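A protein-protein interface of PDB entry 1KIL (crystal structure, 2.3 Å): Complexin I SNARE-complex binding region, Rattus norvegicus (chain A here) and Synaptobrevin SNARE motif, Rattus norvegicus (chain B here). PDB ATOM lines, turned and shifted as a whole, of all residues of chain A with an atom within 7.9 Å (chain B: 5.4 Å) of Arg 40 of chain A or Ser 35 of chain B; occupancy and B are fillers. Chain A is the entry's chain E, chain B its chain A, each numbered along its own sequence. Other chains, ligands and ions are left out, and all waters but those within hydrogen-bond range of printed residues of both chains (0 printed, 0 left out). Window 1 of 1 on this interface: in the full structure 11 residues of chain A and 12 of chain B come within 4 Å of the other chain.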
ATOM      1  N   TYR A  29      24.798   1.679  -4.508  1.00  0.00           N
ATOM      2  CA  TYR A  29      24.874   3.016  -5.058  1.00  0.00           C
ATOM      3  C   TYR A  29      25.167   2.971  -6.554  1.00  0.00           C
ATOM      4  O   TYR A  29      24.905   3.928  -7.286  1.00  0.00           O
ATOM      5  CB  TYR A  29      25.920   3.840  -4.295  1.00  0.00           C
ATOM      6  CG  TYR A  29      25.306   4.736  -3.227  1.00  0.00           C
ATOM      7  CD1 TYR A  29      24.645   5.908  -3.576  1.00  0.00           C
ATOM      8  CD2 TYR A  29      25.313   4.368  -1.883  1.00  0.00           C
ATOM      9  CE1 TYR A  29      24.004   6.689  -2.623  1.00  0.00           C
ATOM     10  CE2 TYR A  29      24.672   5.144  -0.915  1.00  0.00           C
ATOM     11  CZ  TYR A  29      24.016   6.302  -1.291  1.00  0.00           C
ATOM     12  OH  TYR A  29      23.336   7.056  -0.352  1.00  0.00           O
ATOM     13  N   ALA A  30      25.696   1.850  -7.023  1.00  0.00           N
ATOM     14  CA  ALA A  30      25.984   1.729  -8.443  1.00  0.00           C
ATOM     15  C   ALA A  30      24.673   1.442  -9.177  1.00  0.00           C
ATOM     16  O   ALA A  30      24.460   1.917 -10.297  1.00  0.00           O
ATOM     17  CB  ALA A  30      26.991   0.624  -8.682  1.00  0.00           C
ATOM     18  N   MET A  32      21.772   2.494  -8.169  1.00  0.00           N
ATOM     19  CA  MET A  32      21.030   3.740  -8.116  1.00  0.00           C
ATOM     20  C   MET A  32      21.489   4.640  -9.264  1.00  0.00           C
ATOM     21  O   MET A  32      20.674   5.231  -9.985  1.00  0.00           O
ATOM     22  CB  MET A  32      21.253   4.443  -6.769  1.00  0.00           C
ATOM     23  CG  MET A  32      20.573   3.774  -5.561  1.00  0.00           C
ATOM     24  SD  MET A  32      20.809   4.659  -3.939  1.00  0.00           S
ATOM     25  CE  MET A  32      21.445   3.381  -2.873  1.00  0.00           C
ATOM     26  N   GLU A  33      22.800   4.717  -9.452  1.00  0.00           N
ATOM     27  CA  GLU A  33      23.354   5.562 -10.502  1.00  0.00           C
ATOM     28  C   GLU A  33      22.850   5.160 -11.899  1.00  0.00           C
ATOM     29  O   GLU A  33      22.413   6.019 -12.678  1.00  0.00           O
ATOM     30  CB  GLU A  33      24.891   5.541 -10.436  1.00  0.00           C
ATOM     31  CG  GLU A  33      25.608   6.253 -11.600  1.00  0.00           C
ATOM     32  CD  GLU A  33      25.118   7.680 -11.820  1.00  0.00           C
ATOM     33  OE1 GLU A  33      24.393   8.191 -10.954  1.00  0.00           O
ATOM     34  OE2 GLU A  33      25.453   8.292 -12.856  1.00  0.00           O
ATOM     35  N   ALA A  34      22.890   3.861 -12.206  1.00  0.00           N
ATOM     36  CA  ALA A  34      22.431   3.364 -13.511  1.00  0.00           C
ATOM     37  C   ALA A  34      20.975   3.759 -13.724  1.00  0.00           C
ATOM     38  O   ALA A  34      20.582   4.220 -14.800  1.00  0.00           O
ATOM     39  CB  ALA A  34      22.574   1.852 -13.589  1.00  0.00           C
ATOM     40  N   GLU A  35      20.171   3.590 -12.686  1.00  0.00           N
ATOM     41  CA  GLU A  35      18.776   3.948 -12.805  1.00  0.00           C
ATOM     42  C   GLU A  35      18.635   5.457 -13.063  1.00  0.00           C
ATOM     43  O   GLU A  35      17.746   5.879 -13.785  1.00  0.00           O
ATOM     44  CB  GLU A  35      18.009   3.538 -11.544  1.00  0.00           C
ATOM     45  CG  GLU A  35      16.508   3.535 -11.742  1.00  0.00           C
ATOM     46  CD  GLU A  35      15.740   3.878 -10.473  1.00  0.00           C
ATOM     47  OE1 GLU A  35      16.257   3.589  -9.365  1.00  0.00           O
ATOM     48  OE2 GLU A  35      14.613   4.422 -10.592  1.00  0.00           O
ATOM     49  N   ARG A  36      19.516   6.277 -12.501  1.00  0.00           N
ATOM     50  CA  ARG A  36      19.401   7.723 -12.737  1.00  0.00           C
ATOM     51  C   ARG A  36      19.781   8.044 -14.168  1.00  0.00           C
ATOM     52  O   ARG A  36      19.120   8.838 -14.825  1.00  0.00           O
ATOM     53  CB  ARG A  36      20.325   8.527 -11.818  1.00  0.00           C
ATOM     54  CG  ARG A  36      20.318   8.126 -10.360  1.00  0.00           C
ATOM     55  CD  ARG A  36      19.349   8.964  -9.561  1.00  0.00           C
ATOM     56  NE  ARG A  36      19.283  10.369  -9.981  1.00  0.00           N
ATOM     57  CZ  ARG A  36      18.385  11.225  -9.505  1.00  0.00           C
ATOM     58  NH1 ARG A  36      17.508  10.815  -8.592  1.00  0.00           N
ATOM     59  NH2 ARG A  36      18.326  12.461  -9.968  1.00  0.00           N
ATOM     60  N   GLU A  37      20.862   7.432 -14.638  1.00  0.00           N
ATOM     61  CA  GLU A  37      21.357   7.657 -15.996  1.00  0.00           C
ATOM     62  C   GLU A  37      20.320   7.300 -17.072  1.00  0.00           C
ATOM     63  O   GLU A  37      20.266   7.931 -18.130  1.00  0.00           O
ATOM     64  CB  GLU A  37      22.663   6.872 -16.201  1.00  0.00           C
ATOM     65  CG  GLU A  37      23.364   7.047 -17.564  1.00  0.00           C
ATOM     66  CD  GLU A  37      23.568   8.502 -18.029  1.00  0.00           C
ATOM     67  OE1 GLU A  37      23.982   9.383 -17.221  1.00  0.00           O
ATOM     68  OE2 GLU A  37      23.333   8.746 -19.245  1.00  0.00           O
ATOM     69  N   VAL A  38      19.487   6.304 -16.799  1.00  0.00           N
ATOM     70  CA  VAL A  38      18.464   5.925 -17.753  1.00  0.00           C
ATOM     71  C   VAL A  38      17.504   7.084 -17.931  1.00  0.00           C
ATOM     72  O   VAL A  38      17.142   7.435 -19.064  1.00  0.00           O
ATOM     73  CB  VAL A  38      17.662   4.694 -17.285  1.00  0.00           C
ATOM     74  CG1 VAL A  38      16.437   4.525 -18.155  1.00  0.00           C
ATOM     75  CG2 VAL A  38      18.527   3.438 -17.360  1.00  0.00           C
ATOM     76  N   MET A  39      17.070   7.664 -16.815  1.00  0.00           N
ATOM     77  CA  MET A  39      16.159   8.798 -16.857  1.00  0.00           C
ATOM     78  C   MET A  39      16.853  10.005 -17.492  1.00  0.00           C
ATOM     79  O   MET A  39      16.210  10.774 -18.202  1.00  0.00           O
ATOM     80  CB  MET A  39      15.644   9.132 -15.445  1.00  0.00           C
ATOM     81  CG  MET A  39      15.116  10.563 -15.263  1.00  0.00           C
ATOM     82  SD  MET A  39      16.414  11.707 -14.778  1.00  0.00           S
ATOM     83  CE  MET A  39      16.441  12.808 -16.103  1.00  0.00           C
ATOM     84  N   ARG A  40      18.160  10.151 -17.264  1.00  0.00           N
ATOM     85  CA  ARG A  40      18.920  11.254 -17.839  1.00  0.00           C
ATOM     86  C   ARG A  40      18.961  11.133 -19.350  1.00  0.00           C
ATOM     87  O   ARG A  40      18.843  12.122 -20.074  1.00  0.00           O
ATOM     88  CB  ARG A  40      20.360  11.255 -17.333  1.00  0.00           C
ATOM     89  CG  ARG A  40      20.502  11.508 -15.866  1.00  0.00           C
ATOM     90  CD  ARG A  40      21.968  11.600 -15.474  1.00  0.00           C
ATOM     91  NE  ARG A  40      22.082  11.588 -14.027  1.00  0.00           N
ATOM     92  CZ  ARG A  40      22.894  10.794 -13.339  1.00  0.00           C
ATOM     93  NH1 ARG A  40      23.687   9.938 -13.971  1.00  0.00           N
ATOM     94  NH2 ARG A  40      22.880  10.837 -12.011  1.00  0.00           N
ATOM     95  N   GLN A  41      19.159   9.906 -19.822  1.00  0.00           N
ATOM     96  CA  GLN A  41      19.222   9.662 -21.247  1.00  0.00           C
ATOM     97  C   GLN A  41      17.853   9.890 -21.843  1.00  0.00           C
ATOM     98  O   GLN A  41      17.734  10.465 -22.914  1.00  0.00           O
ATOM     99  CB  GLN A  41      19.660   8.238 -21.529  1.00  0.00           C
ATOM    100  CG  GLN A  41      19.957   8.026 -22.996  1.00  0.00           C
ATOM    101  CD  GLN A  41      21.007   8.996 -23.495  1.00  0.00           C
ATOM    102  OE1 GLN A  41      22.106   9.061 -22.953  1.00  0.00           O
ATOM    103  NE2 GLN A  41      20.674   9.753 -24.531  1.00  0.00           N
ATOM    104  N   GLY A  42      16.821   9.431 -21.147  1.00  0.00           N
ATOM    105  CA  GLY A  42      15.470   9.618 -21.638  1.00  0.00           C
ATOM    106  C   GLY A  42      15.220  11.087 -21.906  1.00  0.00           C
ATOM    107  O   GLY A  42      14.686  11.451 -22.953  1.00  0.00           O
ATOM    108  N   ILE A  43      15.611  11.930 -20.956  1.00  0.00           N
ATOM    109  CA  ILE A  43      15.455  13.365 -21.077  1.00  0.00           C
ATOM    110  C   ILE A  43      16.364  13.864 -22.207  1.00  0.00           C
ATOM    111  O   ILE A  43      16.015  14.800 -22.933  1.00  0.00           O
ATOM    112  CB  ILE A  43      15.848  14.087 -19.734  1.00  0.00           C
ATOM    113  CG1 ILE A  43      14.725  13.962 -18.705  1.00  0.00           C
ATOM    114  CG2 ILE A  43      16.146  15.566 -19.981  1.00  0.00           C
ATOM    115  CD1 ILE A  43      13.467  14.710 -19.082  1.00  0.00           C
ATOM    116  N   ARG A  44      17.531  13.247 -22.354  1.00  0.00           N
ATOM    117  CA  ARG A  44      18.470  13.661 -23.391  1.00  0.00           C
ATOM    118  C   ARG A  44      17.863  13.506 -24.783  1.00  0.00           C
ATOM    119  O   ARG A  44      17.817  14.466 -25.555  1.00  0.00           O
ATOM    120  CB  ARG A  44      19.772  12.857 -23.292  1.00  0.00           C
ATOM    121  CG  ARG A  44      20.949  13.637 -22.716  1.00  0.00           C
ATOM    122  CD  ARG A  44      22.221  12.826 -22.828  1.00  0.00           C
ATOM    123  NE  ARG A  44      22.407  11.898 -21.718  1.00  0.00           N
ATOM    124  CZ  ARG A  44      22.992  12.218 -20.561  1.00  0.00           C
ATOM    125  NH1 ARG A  44      23.450  13.455 -20.363  1.00  0.00           N
ATOM    126  NH2 ARG A  44      23.134  11.302 -19.603  1.00  0.00           N
ATOM    127  N   ASP A  45      17.391  12.300 -25.092  1.00  0.00           N
ATOM    128  CA  ASP A  45      16.775  12.046 -26.384  1.00  0.00           C
ATOM    129  C   ASP A  45      15.668  13.049 -26.577  1.00  0.00           C
ATOM    130  O   ASP A  45      15.649  13.798 -27.556  1.00  0.00           O
ATOM    131  CB  ASP A  45      16.167  10.648 -26.453  1.00  0.00           C
ATOM    132  CG  ASP A  45      17.194   9.561 -26.284  1.00  0.00           C
ATOM    133  OD1 ASP A  45      18.384   9.813 -26.594  1.00  0.00           O
ATOM    134  OD2 ASP A  45      16.805   8.453 -25.850  1.00  0.00           O
ATOM    135  N   LYS A  46      14.747  13.064 -25.624  1.00  0.00           N
ATOM    136  CA  LYS A  46      13.615  13.963 -25.690  1.00  0.00           C
ATOM    137  C   LYS A  46      13.962  15.362 -26.186  1.00  0.00           C
ATOM    138  O   LYS A  46      13.162  15.987 -26.866  1.00  0.00           O
ATOM    139  CB  LYS A  46      12.947  14.045 -24.320  1.00  0.00           C
ATOM    140  CG  LYS A  46      11.651  14.830 -24.294  1.00  0.00           C
ATOM    141  CD  LYS A  46      11.026  14.806 -22.909  1.00  0.00           C
ATOM    142  CE  LYS A  46       9.762  15.638 -22.848  1.00  0.00           C
ATOM    143  NZ  LYS A  46       9.214  15.682 -21.465  1.00  0.00           N
ATOM    144  N   TYR A  47      15.157  15.854 -25.882  1.00  0.00           N
ATOM    145  CA  TYR A  47      15.499  17.210 -26.312  1.00  0.00           C
ATOM    146  C   TYR A  47      16.712  17.363 -27.212  1.00  0.00           C
ATOM    147  O   TYR A  47      17.116  18.483 -27.532  1.00  0.00           O
ATOM    148  CB  TYR A  47      15.668  18.111 -25.086  1.00  0.00           C
ATOM    149  CG  TYR A  47      14.403  18.253 -24.259  1.00  0.00           C
ATOM    150  CD1 TYR A  47      13.245  18.800 -24.801  1.00  0.00           C
ATOM    151  CD2 TYR A  47      14.373  17.836 -22.935  1.00  0.00           C
ATOM    152  CE1 TYR A  47      12.089  18.937 -24.042  1.00  0.00           C
ATOM    153  CE2 TYR A  47      13.233  17.964 -22.170  1.00  0.00           C
ATOM    154  CZ  TYR A  47      12.090  18.513 -22.721  1.00  0.00           C
ATOM    155  OH  TYR A  47      10.965  18.639 -21.933  1.00  0.00           O
ATOM    156  N   ILE A  49      20.392  16.001 -27.081  1.00  0.00           N
ATOM    157  CA  ILE A  49      21.568  16.338 -26.296  1.00  0.00           C
ATOM    158  C   ILE A  49      22.438  15.091 -26.327  1.00  0.00           C
ATOM    159  O   ILE A  49      23.678  15.226 -26.481  1.00  0.00           O
ATOM    160  CB  ILE A  49      21.175  16.704 -24.852  1.00  0.00           C
ATOM    161  CG1 ILE A  49      20.388  18.023 -24.860  1.00  0.00           C
ATOM    162  CG2 ILE A  49      22.408  16.840 -23.971  1.00  0.00           C
ATOM    163  CD1 ILE A  49      19.723  18.358 -23.550  1.00  0.00           C
ATOM    164  OXT ILE A  49      21.851  13.988 -26.211  1.00  0.00           O
ATOM    165  N   LEU B  28      21.457  18.162 -15.656  1.00  0.00           N
ATOM    166  CA  LEU B  28      21.736  16.740 -15.777  1.00  0.00           C
ATOM    167  C   LEU B  28      23.169  16.527 -15.251  1.00  0.00           C
ATOM    168  O   LEU B  28      23.526  15.433 -14.800  1.00  0.00           O
ATOM    169  CB  LEU B  28      21.586  16.282 -17.227  1.00  0.00           C
ATOM    170  CG  LEU B  28      20.143  16.255 -17.728  1.00  0.00           C
ATOM    171  CD1 LEU B  28      20.125  16.014 -19.237  1.00  0.00           C
ATOM    172  CD2 LEU B  28      19.365  15.155 -16.984  1.00  0.00           C
ATOM    173  N   ARG B  30      24.306  18.440 -12.779  1.00  0.00           N
ATOM    174  CA  ARG B  30      24.021  18.587 -11.368  1.00  0.00           C
ATOM    175  C   ARG B  30      23.569  17.229 -10.834  1.00  0.00           C
ATOM    176  O   ARG B  30      23.974  16.805  -9.747  1.00  0.00           O
ATOM    177  CB  ARG B  30      22.910  19.626 -11.159  1.00  0.00           C
ATOM    178  CG  ARG B  30      22.629  19.977  -9.691  1.00  0.00           C
ATOM    179  CD  ARG B  30      21.639  21.163  -9.561  1.00  0.00           C
ATOM    180  NE  ARG B  30      21.438  21.589  -8.166  1.00  0.00           N
ATOM    181  CZ  ARG B  30      20.409  21.207  -7.409  1.00  0.00           C
ATOM    182  NH1 ARG B  30      19.475  20.394  -7.902  1.00  0.00           N
ATOM    183  NH2 ARG B  30      20.312  21.627  -6.153  1.00  0.00           N
ATOM    184  N   ASP B  31      22.749  16.548 -11.628  1.00  0.00           N
ATOM    185  CA  ASP B  31      22.199  15.244 -11.271  1.00  0.00           C
ATOM    186  C   ASP B  31      23.284  14.197 -11.032  1.00  0.00           C
ATOM    187  O   ASP B  31      23.239  13.436 -10.052  1.00  0.00           O
ATOM    188  CB  ASP B  31      21.259  14.765 -12.378  1.00  0.00           C
ATOM    189  CG  ASP B  31      20.307  13.676 -11.916  1.00  0.00           C
ATOM    190  OD1 ASP B  31      20.701  12.485 -11.844  1.00  0.00           O
ATOM    191  OD2 ASP B  31      19.148  14.025 -11.604  1.00  0.00           O
ATOM    192  N   GLN B  32      24.276  14.176 -11.911  1.00  0.00           N
ATOM    193  CA  GLN B  32      25.338  13.193 -11.804  1.00  0.00           C
ATOM    194  C   GLN B  32      26.269  13.532 -10.651  1.00  0.00           C
ATOM    195  O   GLN B  32      26.733  12.643  -9.932  1.00  0.00           O
ATOM    196  CB  GLN B  32      26.108  13.145 -13.120  1.00  0.00           C
ATOM    197  CG  GLN B  32      26.761  11.809 -13.448  1.00  0.00           C
ATOM    198  CD  GLN B  32      27.400  11.832 -14.824  1.00  0.00           C
ATOM    199  OE1 GLN B  32      26.744  12.156 -15.824  1.00  0.00           O
ATOM    200  NE2 GLN B  32      28.689  11.502 -14.887  1.00  0.00           N
ATOM    201  N   LYS B  33      26.550  14.823 -10.476  1.00  0.00           N
ATOM    202  CA  LYS B  33      27.413  15.238  -9.388  1.00  0.00           C
ATOM    203  C   LYS B  33      26.749  14.913  -8.058  1.00  0.00           C
ATOM    204  O   LYS B  33      27.387  14.374  -7.170  1.00  0.00           O
ATOM    205  CB  LYS B  33      27.707  16.733  -9.459  1.00  0.00           C
ATOM    206  CG  LYS B  33      28.584  17.195 -10.607  1.00  0.00           C
ATOM    207  CD  LYS B  33      28.660  18.724 -10.578  1.00  0.00           C
ATOM    208  CE  LYS B  33      29.199  19.311 -11.857  1.00  0.00           C
ATOM    209  NZ  LYS B  33      30.626  18.898 -11.997  1.00  0.00           N
ATOM    210  N   LEU B  34      25.466  15.231  -7.921  1.00  0.00           N
ATOM    211  CA  LEU B  34      24.763  14.957  -6.677  1.00  0.00           C
ATOM    212  C   LEU B  34      24.707  13.460  -6.401  1.00  0.00           C
ATOM    213  O   LEU B  34      24.790  13.000  -5.248  1.00  0.00           O
ATOM    214  CB  LEU B  34      23.358  15.560  -6.737  1.00  0.00           C
ATOM    215  CG  LEU B  34      23.343  17.079  -6.455  1.00  0.00           C
ATOM    216  CD1 LEU B  34      21.931  17.671  -6.605  1.00  0.00           C
ATOM    217  CD2 LEU B  34      23.907  17.316  -5.040  1.00  0.00           C
ATOM    218  N   SER B  35      24.578  12.693  -7.473  1.00  0.00           N
ATOM    219  CA  SER B  35      24.518  11.256  -7.336  1.00  0.00           C
ATOM    220  C   SER B  35      25.840  10.732  -6.789  1.00  0.00           C
ATOM    221  O   SER B  35      25.900   9.786  -6.015  1.00  0.00           O
ATOM    222  CB  SER B  35      24.238  10.620  -8.683  1.00  0.00           C
ATOM    223  OG  SER B  35      24.090   9.240  -8.495  1.00  0.00           O
ATOM    224  N   GLU B  36      26.914  11.377  -7.189  1.00  0.00           N
ATOM    225  CA  GLU B  36      28.215  10.964  -6.723  1.00  0.00           C
ATOM    226  C   GLU B  36      28.457  11.379  -5.268  1.00  0.00           C
ATOM    227  O   GLU B  36      29.089  10.663  -4.497  1.00  0.00           O
ATOM    228  CB  GLU B  36      29.269  11.580  -7.630  1.00  0.00           C
ATOM    229  CG  GLU B  36      30.690  11.321  -7.191  1.00  0.00           C
ATOM    230  CD  GLU B  36      31.698  11.957  -8.137  1.00  0.00           C
ATOM    231  OE1 GLU B  36      32.866  12.097  -7.721  1.00  0.00           O
ATOM    232  OE2 GLU B  36      31.325  12.316  -9.291  1.00  0.00           O
ATOM    233  N   LEU B  37      27.944  12.550  -4.910  1.00  0.00           N
ATOM    234  CA  LEU B  37      28.101  13.109  -3.585  1.00  0.00           C
ATOM    235  C   LEU B  37      27.238  12.356  -2.589  1.00  0.00           C
ATOM    236  O   LEU B  37      27.583  12.221  -1.430  1.00  0.00           O
ATOM    237  CB  LEU B  37      27.726  14.578  -3.634  1.00  0.00           C
ATOM    238  CG  LEU B  37      27.723  15.320  -2.297  1.00  0.00           C
ATOM    239  CD1 LEU B  37      29.067  15.144  -1.655  1.00  0.00           C
ATOM    240  CD2 LEU B  37      27.398  16.820  -2.527  1.00  0.00           C
ATOM    241  N   ASP B  38      26.106  11.871  -3.050  1.00  0.00           N
ATOM    242  CA  ASP B  38      25.207  11.111  -2.203  1.00  0.00           C
ATOM    243  C   ASP B  38      25.919   9.801  -1.812  1.00  0.00           C
ATOM    244  O   ASP B  38      25.741   9.287  -0.706  1.00  0.00           O
ATOM    245  CB  ASP B  38      23.915  10.843  -2.995  1.00  0.00           C
ATOM    246  CG  ASP B  38      22.843  10.097  -2.193  1.00  0.00           C
ATOM    247  OD1 ASP B  38      22.898  10.009  -0.945  1.00  0.00           O
ATOM    248  OD2 ASP B  38      21.913   9.607  -2.843  1.00  0.00           O
ATOM    249  N   ASP B  39      26.731   9.270  -2.722  1.00  0.00           N
ATOM    250  CA  ASP B  39      27.486   8.034  -2.477  1.00  0.00           C
ATOM    251  C   ASP B  39      28.613   8.389  -1.496  1.00  0.00           C
ATOM    252  O   ASP B  39      28.771   7.758  -0.451  1.00  0.00           O
ATOM    253  CB  ASP B  39      28.047   7.513  -3.814  1.00  0.00           C
ATOM    254  CG  ASP B  39      28.901   6.252  -3.664  1.00  0.00           C
ATOM    255  OD1 ASP B  39      29.439   5.807  -4.696  1.00  0.00           O
ATOM    256  OD2 ASP B  39      29.049   5.691  -2.548  1.00  0.00           O
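The side-chain carboxylate of Asp 31 of chain B is in salt-bridge range of the guanidinium group of Arg 36 of chain A (2.4 Å). NE of Arg 40 of chain A lies within salt-bridge range of OD1 of Asp 31 of chain B. The side-chain carboxylate of Asp 38 of chain B lies within hydrogen-bond range of the side-chain hydroxyl of Tyr 29 of chain A, 3.0 Å away. The side-chain carboxylate of Glu 33 of chain A lies within hydrogen-bond range of the side-chain hydroxyl of Ser 35 of chain B (2.7 Å).
NH1 of Arg 40 of chain A lies within salt-bridge range of OE2 of Glu 33 of chain A. The guanidinium group of Arg 40 of chain A lies within salt-bridge range of the side-chain carboxylate of Glu 37 of chain A (3.3 Å).
Among the printed residues, pairs that only touch across the chains: Arg 40 of chain A with Gln 32 of chain B, Arg 40 of chain A with Ser 35 of chain B, Tyr 29 of chain A with Asp 39 of chain B, Glu 33 of chain A with Gln 32 of chain B, Met 39 of chain A with Leu 28 of chain B and Arg 40 of chain A with Leu 28 of chain B.
Of the printed residues of chain B, Arg 40 of chain A touches Leu 28 (3.98 Å), Asp 31 (2.7 Å), Gln 32 (3.4 Å) and Ser 35 (3.6 Å). Of chain A, only Glu 33 and Arg 40 come within 4 Å of Ser 35 of chain B. Printed residues of chain A within 4 Å of Asp 31 of chain B: Arg 36 (2.4 Å) and Arg 40 (2.7 Å). Of the printed residues of chain B, Arg 36 of chain A touches Asp 31 (2.4 Å). Of the printed residues of chain A, Asp 39 of chain B touches Tyr 29. Printed residues of chain A within 4 Å of Gln 32 of chain B: Glu 33 (3.8 Å) and Arg 40 (3.4 Å). Ala 30 of chain A touches none of the printed residues of chain B. The nearest printed residue of chain B that does not touch Arg 40 of chain A is Lys 33 of chain B (5.6 Å).
Of the 11 printed residues of chain B, 6 touch a printed residue of chain A. Hydrophobic or aromatic side chains of chain B within 4 Å of the printed part of chain A: Leu 28. Hydrophobic or aromatic side chains of chain A that line the printed part of chain B: Tyr 29 and Met 39. Among the printed residues, 10 pairs touch across the chains.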
